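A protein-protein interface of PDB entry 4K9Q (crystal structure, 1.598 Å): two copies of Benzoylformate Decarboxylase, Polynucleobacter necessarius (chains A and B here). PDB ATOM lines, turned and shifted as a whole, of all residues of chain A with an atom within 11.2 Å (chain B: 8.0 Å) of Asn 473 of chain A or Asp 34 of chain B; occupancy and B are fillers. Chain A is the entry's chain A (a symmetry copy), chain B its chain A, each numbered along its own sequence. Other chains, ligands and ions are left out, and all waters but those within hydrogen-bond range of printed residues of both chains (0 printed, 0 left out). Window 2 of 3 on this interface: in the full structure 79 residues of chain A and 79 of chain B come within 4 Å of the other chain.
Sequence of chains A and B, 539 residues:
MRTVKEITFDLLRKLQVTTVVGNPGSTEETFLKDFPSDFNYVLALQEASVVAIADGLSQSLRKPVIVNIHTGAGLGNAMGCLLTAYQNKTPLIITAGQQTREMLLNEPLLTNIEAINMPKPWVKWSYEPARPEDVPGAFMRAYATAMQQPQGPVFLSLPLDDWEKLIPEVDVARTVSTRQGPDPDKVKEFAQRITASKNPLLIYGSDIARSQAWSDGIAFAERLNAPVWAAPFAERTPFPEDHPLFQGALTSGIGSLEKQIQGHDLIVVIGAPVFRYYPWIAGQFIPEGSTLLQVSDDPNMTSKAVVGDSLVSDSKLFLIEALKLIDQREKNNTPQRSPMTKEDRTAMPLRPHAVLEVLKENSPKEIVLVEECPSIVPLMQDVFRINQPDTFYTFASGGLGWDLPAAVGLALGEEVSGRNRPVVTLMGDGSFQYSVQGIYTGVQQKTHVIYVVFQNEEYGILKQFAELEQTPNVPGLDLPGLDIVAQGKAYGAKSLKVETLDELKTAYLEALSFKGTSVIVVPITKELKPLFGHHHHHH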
ATOM      1  N   LEU A 462       7.735 -10.116  15.727  1.00  0.00           N
ATOM      2  CA  LEU A 462       6.823  -8.972  15.866  1.00  0.00           C
ATOM      3  C   LEU A 462       5.773  -9.202  16.957  1.00  0.00           C
ATOM      4  O   LEU A 462       5.293  -8.248  17.575  1.00  0.00           O
ATOM      5  CB  LEU A 462       6.147  -8.618  14.543  1.00  0.00           C
ATOM      6  CG  LEU A 462       7.076  -8.198  13.400  1.00  0.00           C
ATOM      7  CD1 LEU A 462       6.280  -7.749  12.185  1.00  0.00           C
ATOM      8  CD2 LEU A 462       8.053  -7.114  13.852  1.00  0.00           C
ATOM      9  N   LYS A 463       5.413 -10.456  17.201  1.00  0.00           N
ATOM     10  CA  LYS A 463       4.502 -10.756  18.308  1.00  0.00           C
ATOM     11  C   LYS A 463       5.239 -10.631  19.641  1.00  0.00           C
ATOM     12  O   LYS A 463       4.650 -10.246  20.648  1.00  0.00           O
ATOM     13  CB  LYS A 463       3.877 -12.151  18.155  1.00  0.00           C
ATOM     14  CG  LYS A 463       2.934 -12.274  16.956  1.00  0.00           C
ATOM     15  CD  LYS A 463       2.232 -13.621  16.933  1.00  0.00           C
ATOM     16  CE  LYS A 463       1.350 -13.751  15.701  1.00  0.00           C
ATOM     17  NZ  LYS A 463       0.647 -15.071  15.667  1.00  0.00           N
ATOM     18  N   GLN A 464       6.528 -10.962  19.638  1.00  0.00           N
ATOM     19  CA  GLN A 464       7.363 -10.779  20.820  1.00  0.00           C
ATOM     20  C   GLN A 464       7.425  -9.292  21.147  1.00  0.00           C
ATOM     21  O   GLN A 464       7.311  -8.890  22.303  1.00  0.00           O
ATOM     22  CB  GLN A 464       8.772 -11.325  20.585  1.00  0.00           C
ATOM     23  CG  GLN A 464       8.836 -12.849  20.424  1.00  0.00           C
ATOM     24  CD  GLN A 464      10.242 -13.375  20.179  1.00  0.00           C
ATOM     25  OE1 GLN A 464      10.956 -12.914  19.281  1.00  0.00           O
ATOM     26  NE2 GLN A 464      10.649 -14.352  20.983  1.00  0.00           N
ATOM     27  N   PHE A 465       7.612  -8.474  20.118  1.00  0.00           N
ATOM     28  CA  PHE A 465       7.622  -7.027  20.303  1.00  0.00           C
ATOM     29  C   PHE A 465       6.276  -6.479  20.755  1.00  0.00           C
ATOM     30  O   PHE A 465       6.221  -5.557  21.566  1.00  0.00           O
ATOM     31  CB  PHE A 465       8.024  -6.332  19.006  1.00  0.00           C
ATOM     32  CG  PHE A 465       9.441  -5.898  18.977  1.00  0.00           C
ATOM     33  CD1 PHE A 465       9.815  -4.703  19.565  1.00  0.00           C
ATOM     34  CD2 PHE A 465      10.407  -6.677  18.367  1.00  0.00           C
ATOM     35  CE1 PHE A 465      11.140  -4.279  19.537  1.00  0.00           C
ATOM     36  CE2 PHE A 465      11.735  -6.266  18.340  1.00  0.00           C
ATOM     37  CZ  PHE A 465      12.098  -5.064  18.926  1.00  0.00           C
ATOM     38  N   ALA A 466       5.192  -7.018  20.210  1.00  0.00           N
ATOM     39  CA  ALA A 466       3.860  -6.544  20.564  1.00  0.00           C
ATOM     40  C   ALA A 466       3.609  -6.773  22.054  1.00  0.00           C
ATOM     41  O   ALA A 466       2.893  -6.003  22.696  1.00  0.00           O
ATOM     42  CB  ALA A 466       2.796  -7.249  19.733  1.00  0.00           C
ATOM     43  N   GLU A 467       4.200  -7.841  22.587  1.00  0.00           N
ATOM     44  CA  GLU A 467       4.078  -8.198  24.004  1.00  0.00           C
ATOM     45  C   GLU A 467       4.893  -7.247  24.882  1.00  0.00           C
ATOM     46  O   GLU A 467       4.356  -6.595  25.780  1.00  0.00           O
ATOM     47  CB  GLU A 467       4.523  -9.655  24.215  1.00  0.00           C
ATOM     48  CG  GLU A 467       4.685 -10.078  25.673  1.00  0.00           C
ATOM     49  CD  GLU A 467       3.393 -10.580  26.289  1.00  0.00           C
ATOM     50  OE1 GLU A 467       2.365 -10.620  25.576  1.00  0.00           O
ATOM     51  OE2 GLU A 467       3.408 -10.940  27.488  1.00  0.00           O
ATOM     52  N   GLU A 469       6.052  -4.406  24.143  1.00  0.00           N
ATOM     53  CA  GLU A 469       5.700  -3.001  23.963  1.00  0.00           C
ATOM     54  C   GLU A 469       4.197  -2.737  24.064  1.00  0.00           C
ATOM     55  O   GLU A 469       3.733  -1.613  23.855  1.00  0.00           O
ATOM     56  CB  GLU A 469       6.284  -2.456  22.661  1.00  0.00           C
ATOM     57  CG  GLU A 469       7.800  -2.629  22.550  1.00  0.00           C
ATOM     58  CD  GLU A 469       8.577  -1.881  23.627  1.00  0.00           C
ATOM     59  OE1 GLU A 469       8.047  -0.897  24.188  1.00  0.00           O
ATOM     60  OE2 GLU A 469       9.729  -2.276  23.911  1.00  0.00           O
ATOM     61  N   GLN A 470       3.445  -3.766  24.443  1.00  0.00           N
ATOM     62  CA  GLN A 470       2.007  -3.646  24.694  1.00  0.00           C
ATOM     63  C   GLN A 470       1.193  -3.027  23.550  1.00  0.00           C
ATOM     64  O   GLN A 470       0.441  -2.071  23.752  1.00  0.00           O
ATOM     65  CB  GLN A 470       1.765  -2.884  26.002  1.00  0.00           C
ATOM     66  CG  GLN A 470       2.520  -3.473  27.184  1.00  0.00           C
ATOM     67  CD  GLN A 470       2.011  -2.958  28.518  1.00  0.00           C
ATOM     68  OE1 GLN A 470       2.243  -1.804  28.883  1.00  0.00           O
ATOM     69  NE2 GLN A 470       1.303  -3.817  29.251  1.00  0.00           N
ATOM     70  N   THR A 471       1.339  -3.584  22.350  1.00  0.00           N
ATOM     71  CA  THR A 471       0.546  -3.158  21.206  1.00  0.00           C
ATOM     72  C   THR A 471      -0.294  -4.332  20.696  1.00  0.00           C
ATOM     73  O   THR A 471       0.081  -5.009  19.736  1.00  0.00           O
ATOM     74  CB  THR A 471       1.443  -2.633  20.067  1.00  0.00           C
ATOM     75  OG1 THR A 471       2.406  -3.640  19.726  1.00  0.00           O
ATOM     76  CG2 THR A 471       2.168  -1.367  20.498  1.00  0.00           C
ATOM     77  N   PRO A 472      -1.437  -4.583  21.347  1.00  0.00           N
ATOM     78  CA  PRO A 472      -2.312  -5.680  20.938  1.00  0.00           C
ATOM     79  C   PRO A 472      -3.028  -5.349  19.645  1.00  0.00           C
ATOM     80  O   PRO A 472      -3.119  -4.176  19.254  1.00  0.00           O
ATOM     81  CB  PRO A 472      -3.327  -5.759  22.085  1.00  0.00           C
ATOM     82  CG  PRO A 472      -3.382  -4.371  22.618  1.00  0.00           C
ATOM     83  CD  PRO A 472      -1.978  -3.842  22.501  1.00  0.00           C
ATOM     84  N   ASN A 473      -3.518  -6.390  18.986  1.00  0.00           N
ATOM     85  CA  ASN A 473      -4.388  -6.246  17.829  1.00  0.00           C
ATOM     86  C   ASN A 473      -3.716  -5.570  16.644  1.00  0.00           C
ATOM     87  O   ASN A 473      -4.363  -4.866  15.877  1.00  0.00           O
ATOM     88  CB  ASN A 473      -5.687  -5.536  18.214  1.00  0.00           C
ATOM     89  CG  ASN A 473      -6.464  -6.293  19.287  1.00  0.00           C
ATOM     90  OD1 ASN A 473      -6.607  -7.517  19.221  1.00  0.00           O
ATOM     91  ND2 ASN A 473      -6.941  -5.570  20.292  1.00  0.00           N
ATOM     92  N   VAL A 474      -2.417  -5.806  16.497  1.00  0.00           N
ATOM     93  CA  VAL A 474      -1.708  -5.404  15.287  1.00  0.00           C
ATOM     94  C   VAL A 474      -2.039  -6.399  14.160  1.00  0.00           C
ATOM     95  O   VAL A 474      -1.938  -7.609  14.355  1.00  0.00           O
ATOM     96  CB  VAL A 474      -0.186  -5.371  15.520  1.00  0.00           C
ATOM     97  CG1 VAL A 474       0.565  -5.144  14.202  1.00  0.00           C
ATOM     98  CG2 VAL A 474       0.173  -4.301  16.545  1.00  0.00           C
ATOM     99  N   PRO A 475      -2.462  -5.895  12.987  1.00  0.00           N
ATOM    100  CA  PRO A 475      -2.770  -6.800  11.876  1.00  0.00           C
ATOM    101  C   PRO A 475      -1.531  -7.269  11.125  1.00  0.00           C
ATOM    102  O   PRO A 475      -0.440  -6.741  11.329  1.00  0.00           O
ATOM    103  CB  PRO A 475      -3.645  -5.946  10.957  1.00  0.00           C
ATOM    104  CG  PRO A 475      -3.216  -4.554  11.222  1.00  0.00           C
ATOM    105  CD  PRO A 475      -2.755  -4.485  12.657  1.00  0.00           C
ATOM    106  N   GLY A 476      -1.709  -8.273  10.273  1.00  0.00           N
ATOM    107  CA  GLY A 476      -0.644  -8.728   9.391  1.00  0.00           C
ATOM    108  C   GLY A 476       0.512  -9.499  10.014  1.00  0.00           C
ATOM    109  O   GLY A 476       1.593  -9.569   9.421  1.00  0.00           O
ATOM    110  N   LEU A 477       0.294 -10.109  11.178  1.00  0.00           N
ATOM    111  CA  LEU A 477       1.379 -10.817  11.845  1.00  0.00           C
ATOM    112  C   LEU A 477       1.362 -12.321  11.589  1.00  0.00           C
ATOM    113  O   LEU A 477       2.352 -13.014  11.856  1.00  0.00           O
ATOM    114  CB  LEU A 477       1.388 -10.513  13.347  1.00  0.00           C
ATOM    115  CG  LEU A 477       1.536  -9.036  13.747  1.00  0.00           C
ATOM    116  CD1 LEU A 477       1.697  -8.904  15.255  1.00  0.00           C
ATOM    117  CD2 LEU A 477       2.708  -8.390  13.015  1.00  0.00           C
ATOM    118  N   ASP A 478       0.249 -12.823  11.063  1.00  0.00           N
ATOM    119  CA  ASP A 478       0.123 -14.256  10.761  1.00  0.00           C
ATOM    120  C   ASP A 478       0.356 -14.558   9.287  1.00  0.00           C
ATOM    121  O   ASP A 478      -0.019 -13.770   8.417  1.00  0.00           O
ATOM    122  CB  ASP A 478      -1.240 -14.781  11.202  1.00  0.00           C
ATOM    123  CG  ASP A 478      -1.380 -14.800  12.709  1.00  0.00           C
ATOM    124  OD1 ASP A 478      -0.495 -15.382  13.372  1.00  0.00           O
ATOM    125  OD2 ASP A 478      -2.354 -14.221  13.224  1.00  0.00           O
ATOM    126  N   LYS B   5      -2.635   9.149  17.844  1.00  0.00           N
ATOM    127  CA  LYS B   5      -3.239   8.090  17.041  1.00  0.00           C
ATOM    128  C   LYS B   5      -4.751   8.298  16.853  1.00  0.00           C
ATOM    129  O   LYS B   5      -5.261   8.222  15.730  1.00  0.00           O
ATOM    130  CB  LYS B   5      -2.949   6.706  17.638  1.00  0.00           C
ATOM    131  CG  LYS B   5      -3.480   5.552  16.782  1.00  0.00           C
ATOM    132  CD  LYS B   5      -2.874   4.214  17.189  1.00  0.00           C
ATOM    133  CE  LYS B   5      -3.332   3.766  18.571  1.00  0.00           C
ATOM    134  NZ  LYS B   5      -4.755   3.330  18.592  1.00  0.00           N
ATOM    135  N   PHE B   9      -6.407   8.986  13.126  1.00  0.00           N
ATOM    136  CA  PHE B   9      -7.371   8.095  12.504  1.00  0.00           C
ATOM    137  C   PHE B   9      -8.700   8.816  12.262  1.00  0.00           C
ATOM    138  O   PHE B   9      -9.345   8.604  11.226  1.00  0.00           O
ATOM    139  CB  PHE B   9      -7.539   6.798  13.305  1.00  0.00           C
ATOM    140  CG  PHE B   9      -6.518   5.753  12.960  1.00  0.00           C
ATOM    141  CD1 PHE B   9      -6.760   4.841  11.945  1.00  0.00           C
ATOM    142  CD2 PHE B   9      -5.308   5.693  13.632  1.00  0.00           C
ATOM    143  CE1 PHE B   9      -5.810   3.880  11.611  1.00  0.00           C
ATOM    144  CE2 PHE B   9      -4.357   4.739  13.303  1.00  0.00           C
ATOM    145  CZ  PHE B   9      -4.611   3.834  12.293  1.00  0.00           C
ATOM    146  N   ARG B  13     -10.581   9.288   8.674  1.00  0.00           N
ATOM    147  CA  ARG B  13     -12.004   9.042   8.445  1.00  0.00           C
ATOM    148  C   ARG B  13     -12.651  10.210   7.716  1.00  0.00           C
ATOM    149  O   ARG B  13     -13.392  10.014   6.751  1.00  0.00           O
ATOM    150  CB  ARG B  13     -12.737   8.824   9.769  1.00  0.00           C
ATOM    151  CG  ARG B  13     -12.490   7.471  10.366  1.00  0.00           C
ATOM    152  CD  ARG B  13     -13.289   7.289  11.655  1.00  0.00           C
ATOM    153  NE  ARG B  13     -12.939   6.011  12.247  1.00  0.00           N
ATOM    154  CZ  ARG B  13     -12.039   5.858  13.204  1.00  0.00           C
ATOM    155  NH1 ARG B  13     -11.413   6.913  13.710  1.00  0.00           N
ATOM    156  NH2 ARG B  13     -11.771   4.645  13.655  1.00  0.00           N
ATOM    157  N   GLU B  29       4.279  -0.787  14.958  1.00  0.00           N
ATOM    158  CA  GLU B  29       3.287  -1.431  15.818  1.00  0.00           C
ATOM    159  C   GLU B  29       2.458  -0.443  16.646  1.00  0.00           C
ATOM    160  O   GLU B  29       1.273  -0.673  16.878  1.00  0.00           O
ATOM    161  CB  GLU B  29       3.949  -2.488  16.700  1.00  0.00           C
ATOM    162  CG  GLU B  29       4.390  -3.697  15.893  1.00  0.00           C
ATOM    163  CD  GLU B  29       4.914  -4.834  16.740  1.00  0.00           C
ATOM    164  OE1 GLU B  29       5.455  -4.588  17.840  1.00  0.00           O
ATOM    165  OE2 GLU B  29       4.766  -5.984  16.301  1.00  0.00           O
ATOM    166  N   THR B  30       3.069   0.658  17.077  1.00  0.00           N
ATOM    167  CA  THR B  30       2.329   1.664  17.834  1.00  0.00           C
ATOM    168  C   THR B  30       1.290   2.390  16.967  1.00  0.00           C
ATOM    169  O   THR B  30       0.268   2.860  17.465  1.00  0.00           O
ATOM    170  CB  THR B  30       3.281   2.672  18.498  1.00  0.00           C
ATOM    171  OG1 THR B  30       4.234   3.131  17.532  1.00  0.00           O
ATOM    172  CG2 THR B  30       4.034   1.997  19.637  1.00  0.00           C
ATOM    173  N   PHE B  31       1.563   2.481  15.669  1.00  0.00           N
ATOM    174  CA  PHE B  31       0.585   3.016  14.721  1.00  0.00           C
ATOM    175  C   PHE B  31      -0.563   2.029  14.498  1.00  0.00           C
ATOM    176  O   PHE B  31      -1.727   2.421  14.387  1.00  0.00           O
ATOM    177  CB  PHE B  31       1.272   3.331  13.387  1.00  0.00           C
ATOM    178  CG  PHE B  31       0.322   3.689  12.281  1.00  0.00           C
ATOM    179  CD1 PHE B  31      -0.450   4.837  12.355  1.00  0.00           C
ATOM    180  CD2 PHE B  31       0.208   2.875  11.157  1.00  0.00           C
ATOM    181  CE1 PHE B  31      -1.321   5.176  11.333  1.00  0.00           C
ATOM    182  CE2 PHE B  31      -0.663   3.207  10.119  1.00  0.00           C
ATOM    183  CZ  PHE B  31      -1.432   4.354  10.209  1.00  0.00           C
ATOM    184  N   LEU B  32      -0.228   0.741  14.450  1.00  0.00           N
ATOM    185  CA  LEU B  32      -1.192  -0.297  14.101  1.00  0.00           C
ATOM    186  C   LEU B  32      -1.916  -0.908  15.299  1.00  0.00           C
ATOM    187  O   LEU B  32      -2.844  -1.684  15.126  1.00  0.00           O
ATOM    188  CB  LEU B  32      -0.488  -1.412  13.327  1.00  0.00           C
ATOM    189  CG  LEU B  32       0.155  -1.000  11.996  1.00  0.00           C
ATOM    190  CD1 LEU B  32       0.947  -2.159  11.443  1.00  0.00           C
ATOM    191  CD2 LEU B  32      -0.889  -0.535  10.984  1.00  0.00           C
ATOM    192  N   LYS B  33      -1.489  -0.561  16.507  1.00  0.00           N
ATOM    193  CA  LYS B  33      -2.145  -1.040  17.718  1.00  0.00           C
ATOM    194  C   LYS B  33      -3.654  -0.795  17.673  1.00  0.00           C
ATOM    195  O   LYS B  33      -4.098   0.301  17.326  1.00  0.00           O
ATOM    196  CB  LYS B  33      -1.524  -0.338  18.932  1.00  0.00           C
ATOM    197  CG  LYS B  33      -2.268  -0.545  20.241  1.00  0.00           C
ATOM    198  CD  LYS B  33      -1.517   0.147  21.373  1.00  0.00           C
ATOM    199  CE  LYS B  33      -2.283   0.087  22.677  1.00  0.00           C
ATOM    200  NZ  LYS B  33      -3.539   0.877  22.607  1.00  0.00           N
ATOM    201  N   ASP B  34      -4.431  -1.816  18.030  1.00  0.00           N
ATOM    202  CA  ASP B  34      -5.891  -1.733  18.022  1.00  0.00           C
ATOM    203  C   ASP B  34      -6.419  -1.183  16.696  1.00  0.00           C
ATOM    204  O   ASP B  34      -7.313  -0.340  16.672  1.00  0.00           O
ATOM    205  CB  ASP B  34      -6.382  -0.865  19.180  1.00  0.00           C
ATOM    206  CG  ASP B  34      -6.114  -1.492  20.538  1.00  0.00           C
ATOM    207  OD1 ASP B  34      -6.218  -2.730  20.651  1.00  0.00           O
ATOM    208  OD2 ASP B  34      -5.798  -0.744  21.488  1.00  0.00           O
ATOM    209  N   PHE B  35      -5.856  -1.662  15.594  1.00  0.00           N
ATOM    210  CA  PHE B  35      -6.268  -1.204  14.277  1.00  0.00           C
ATOM    211  C   PHE B  35      -7.795  -1.243  14.186  1.00  0.00           C
ATOM    212  O   PHE B  35      -8.412  -2.260  14.503  1.00  0.00           O
ATOM    213  CB  PHE B  35      -5.634  -2.071  13.191  1.00  0.00           C
ATOM    214  CG  PHE B  35      -5.685  -1.446  11.829  1.00  0.00           C
ATOM    215  CD1 PHE B  35      -6.663  -1.812  10.919  1.00  0.00           C
ATOM    216  CD2 PHE B  35      -4.767  -0.474  11.471  1.00  0.00           C
ATOM    217  CE1 PHE B  35      -6.712  -1.227   9.664  1.00  0.00           C
ATOM    218  CE2 PHE B  35      -4.815   0.120  10.224  1.00  0.00           C
ATOM    219  CZ  PHE B  35      -5.790  -0.259   9.322  1.00  0.00           C
ATOM    220  N   PRO B  36      -8.416  -0.117  13.800  1.00  0.00           N
ATOM    221  CA  PRO B  36      -9.879  -0.064  13.916  1.00  0.00           C
ATOM    222  C   PRO B  36     -10.599  -0.844  12.831  1.00  0.00           C
ATOM    223  O   PRO B  36     -10.107  -0.983  11.708  1.00  0.00           O
ATOM    224  CB  PRO B  36     -10.192   1.432  13.811  1.00  0.00           C
ATOM    225  CG  PRO B  36      -9.033   2.025  13.101  1.00  0.00           C
ATOM    226  CD  PRO B  36      -7.831   1.189  13.456  1.00  0.00           C
ATOM    227  N   SER B  37     -11.776  -1.346  13.187  1.00  0.00           N
ATOM    228  CA  SER B  37     -12.544  -2.232  12.326  1.00  0.00           C
ATOM    229  C   SER B  37     -13.130  -1.538  11.108  1.00  0.00           C
ATOM    230  O   SER B  37     -13.510  -2.200  10.135  1.00  0.00           O
ATOM    231  CB  SER B  37     -13.670  -2.884  13.137  1.00  0.00           C
ATOM    232  OG  SER B  37     -14.373  -1.896  13.868  1.00  0.00           O
ATOM    233  N   ASP B  38     -13.216  -0.211  11.147  1.00  0.00           N
ATOM    234  CA  ASP B  38     -13.735   0.506   9.990  1.00  0.00           C
ATOM    235  C   ASP B  38     -12.640   0.893   8.995  1.00  0.00           C
ATOM    236  O   ASP B  38     -12.915   1.530   7.986  1.00  0.00           O
ATOM    237  CB  ASP B  38     -14.592   1.713  10.395  1.00  0.00           C
ATOM    238  CG  ASP B  38     -13.827   2.751  11.199  1.00  0.00           C
ATOM    239  OD1 ASP B  38     -12.867   2.406  11.918  1.00  0.00           O
ATOM    240  OD2 ASP B  38     -14.217   3.931  11.123  1.00  0.00           O
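Among the printed residues, pairs that only touch across the chains: Phe 465 of chain A with Glu 29 of chain B, Gln 470 of chain A with Lys 33 of chain B, Thr 471 of chain A with Glu 29 of chain B, Thr 471 of chain A with Thr 30 of chain B, Thr 471 of chain A with Lys 33 of chain B, Pro 472 of chain A with Lys 33 of chain B, Asn 473 of chain A with Leu 32 of chain B, Asn 473 of chain A with Phe 35 of chain B, Val 474 of chain A with Glu 29 of chain B, Val 474 of chain A with Leu 32 of chain B, Pro 475 of chain A with Leu 32 of chain B and Pro 475 of chain A with Phe 35 of chain B.
Hydrophobic or aromatic side chains of chain A that line the printed part of chain B: Leu 462, Phe 465, Pro 472, Val 474 and Pro 475. Among the printed residues, no Asp or Glu carboxylate lies within 4 Å of a Lys or Arg side-chain nitrogen of the other chain.
No position is printed for both chains. Of the 16 pairs that touch across the chains among the printed residues, none has its exchanged pair printed and touching as well.
Printed residues of chain B within 4 Å of Leu 462 of chain A: Glu 29 (2.7 Å). Lys 463 of chain A touches none of the printed residues of chain B. Of the printed residues of chain B, Thr 471 of chain A touches Glu 29 (3.6 Å), Thr 30 (3.9 Å) and Lys 33 (3.9 Å). Of the printed residues of chain B, Pro 472 of chain A touches Lys 33 (3.6 Å) and Asp 34 (3.0 Å). Of chain B, only Leu 32, Asp 34 and Phe 35 come within 4 Å of Asn 473 of chain A. Printed residues of chain B within 4 Å of Val 474 of chain A: Glu 29 and Leu 32. Printed residues of chain A within 4 Å of Thr 30 of chain B: Thr 471. Phe 31 of chain B touches none of the printed residues of chain A. Of chain A, only Gln 470 (3.6 Å), Thr 471 (3.9 Å) and Pro 472 (3.6 Å) come within 4 Å of Lys 33 of chain B. No residue of chain A comes within 4 Å of Pro 36 of chain B. The nearest residue of chain B that does not touch Asn 473 of chain A is Lys 33 of chain B (4.5 Å). The nearest residue of chain A that does not touch Asp 34 of chain B is Val 474 of chain A (4.7 Å). The nearest printed residue of chain B that does not touch Val 474 of chain A is Lys 33 of chain B (4.1 Å).
The side-chain amino group (NZ) of Lys 5 of chain B sits at hydrogen-bond distance from the backbone carbonyl oxygen (O) of Lys 33 of chain B (3.3 Å). The side-chain amino group (NZ) of Lys 33 of chain B lies within salt-bridge range of the side-chain carboxylate (OD2) of Asp 34 of chain B. The backbone carbonyl oxygen (O) of Ala 466 of chain A is in hydrogen-bond range of the backbone NH (N) of Thr 471 of chain A, at 2.9 Å.
O of Leu 462 of chain A lies close to OE2 of Glu 29 of chain B (2.7 Å). The side-chain carboxylate of Glu 29 of chain B is in hydrogen-bond range of the backbone NH of Ala 466 of chain A. The backbone NH (N) of Asp 34 of chain B is in hydrogen-bond range of the backbone carbonyl oxygen (O) of Pro 472 of chain A (3.0 Å). The side-chain amide nitrogen (ND2) of Asn 473 of chain A sits at hydrogen-bond distance from the side-chain carboxylate (OD1) of Asp 34 of chain B, 3.0 Å away.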
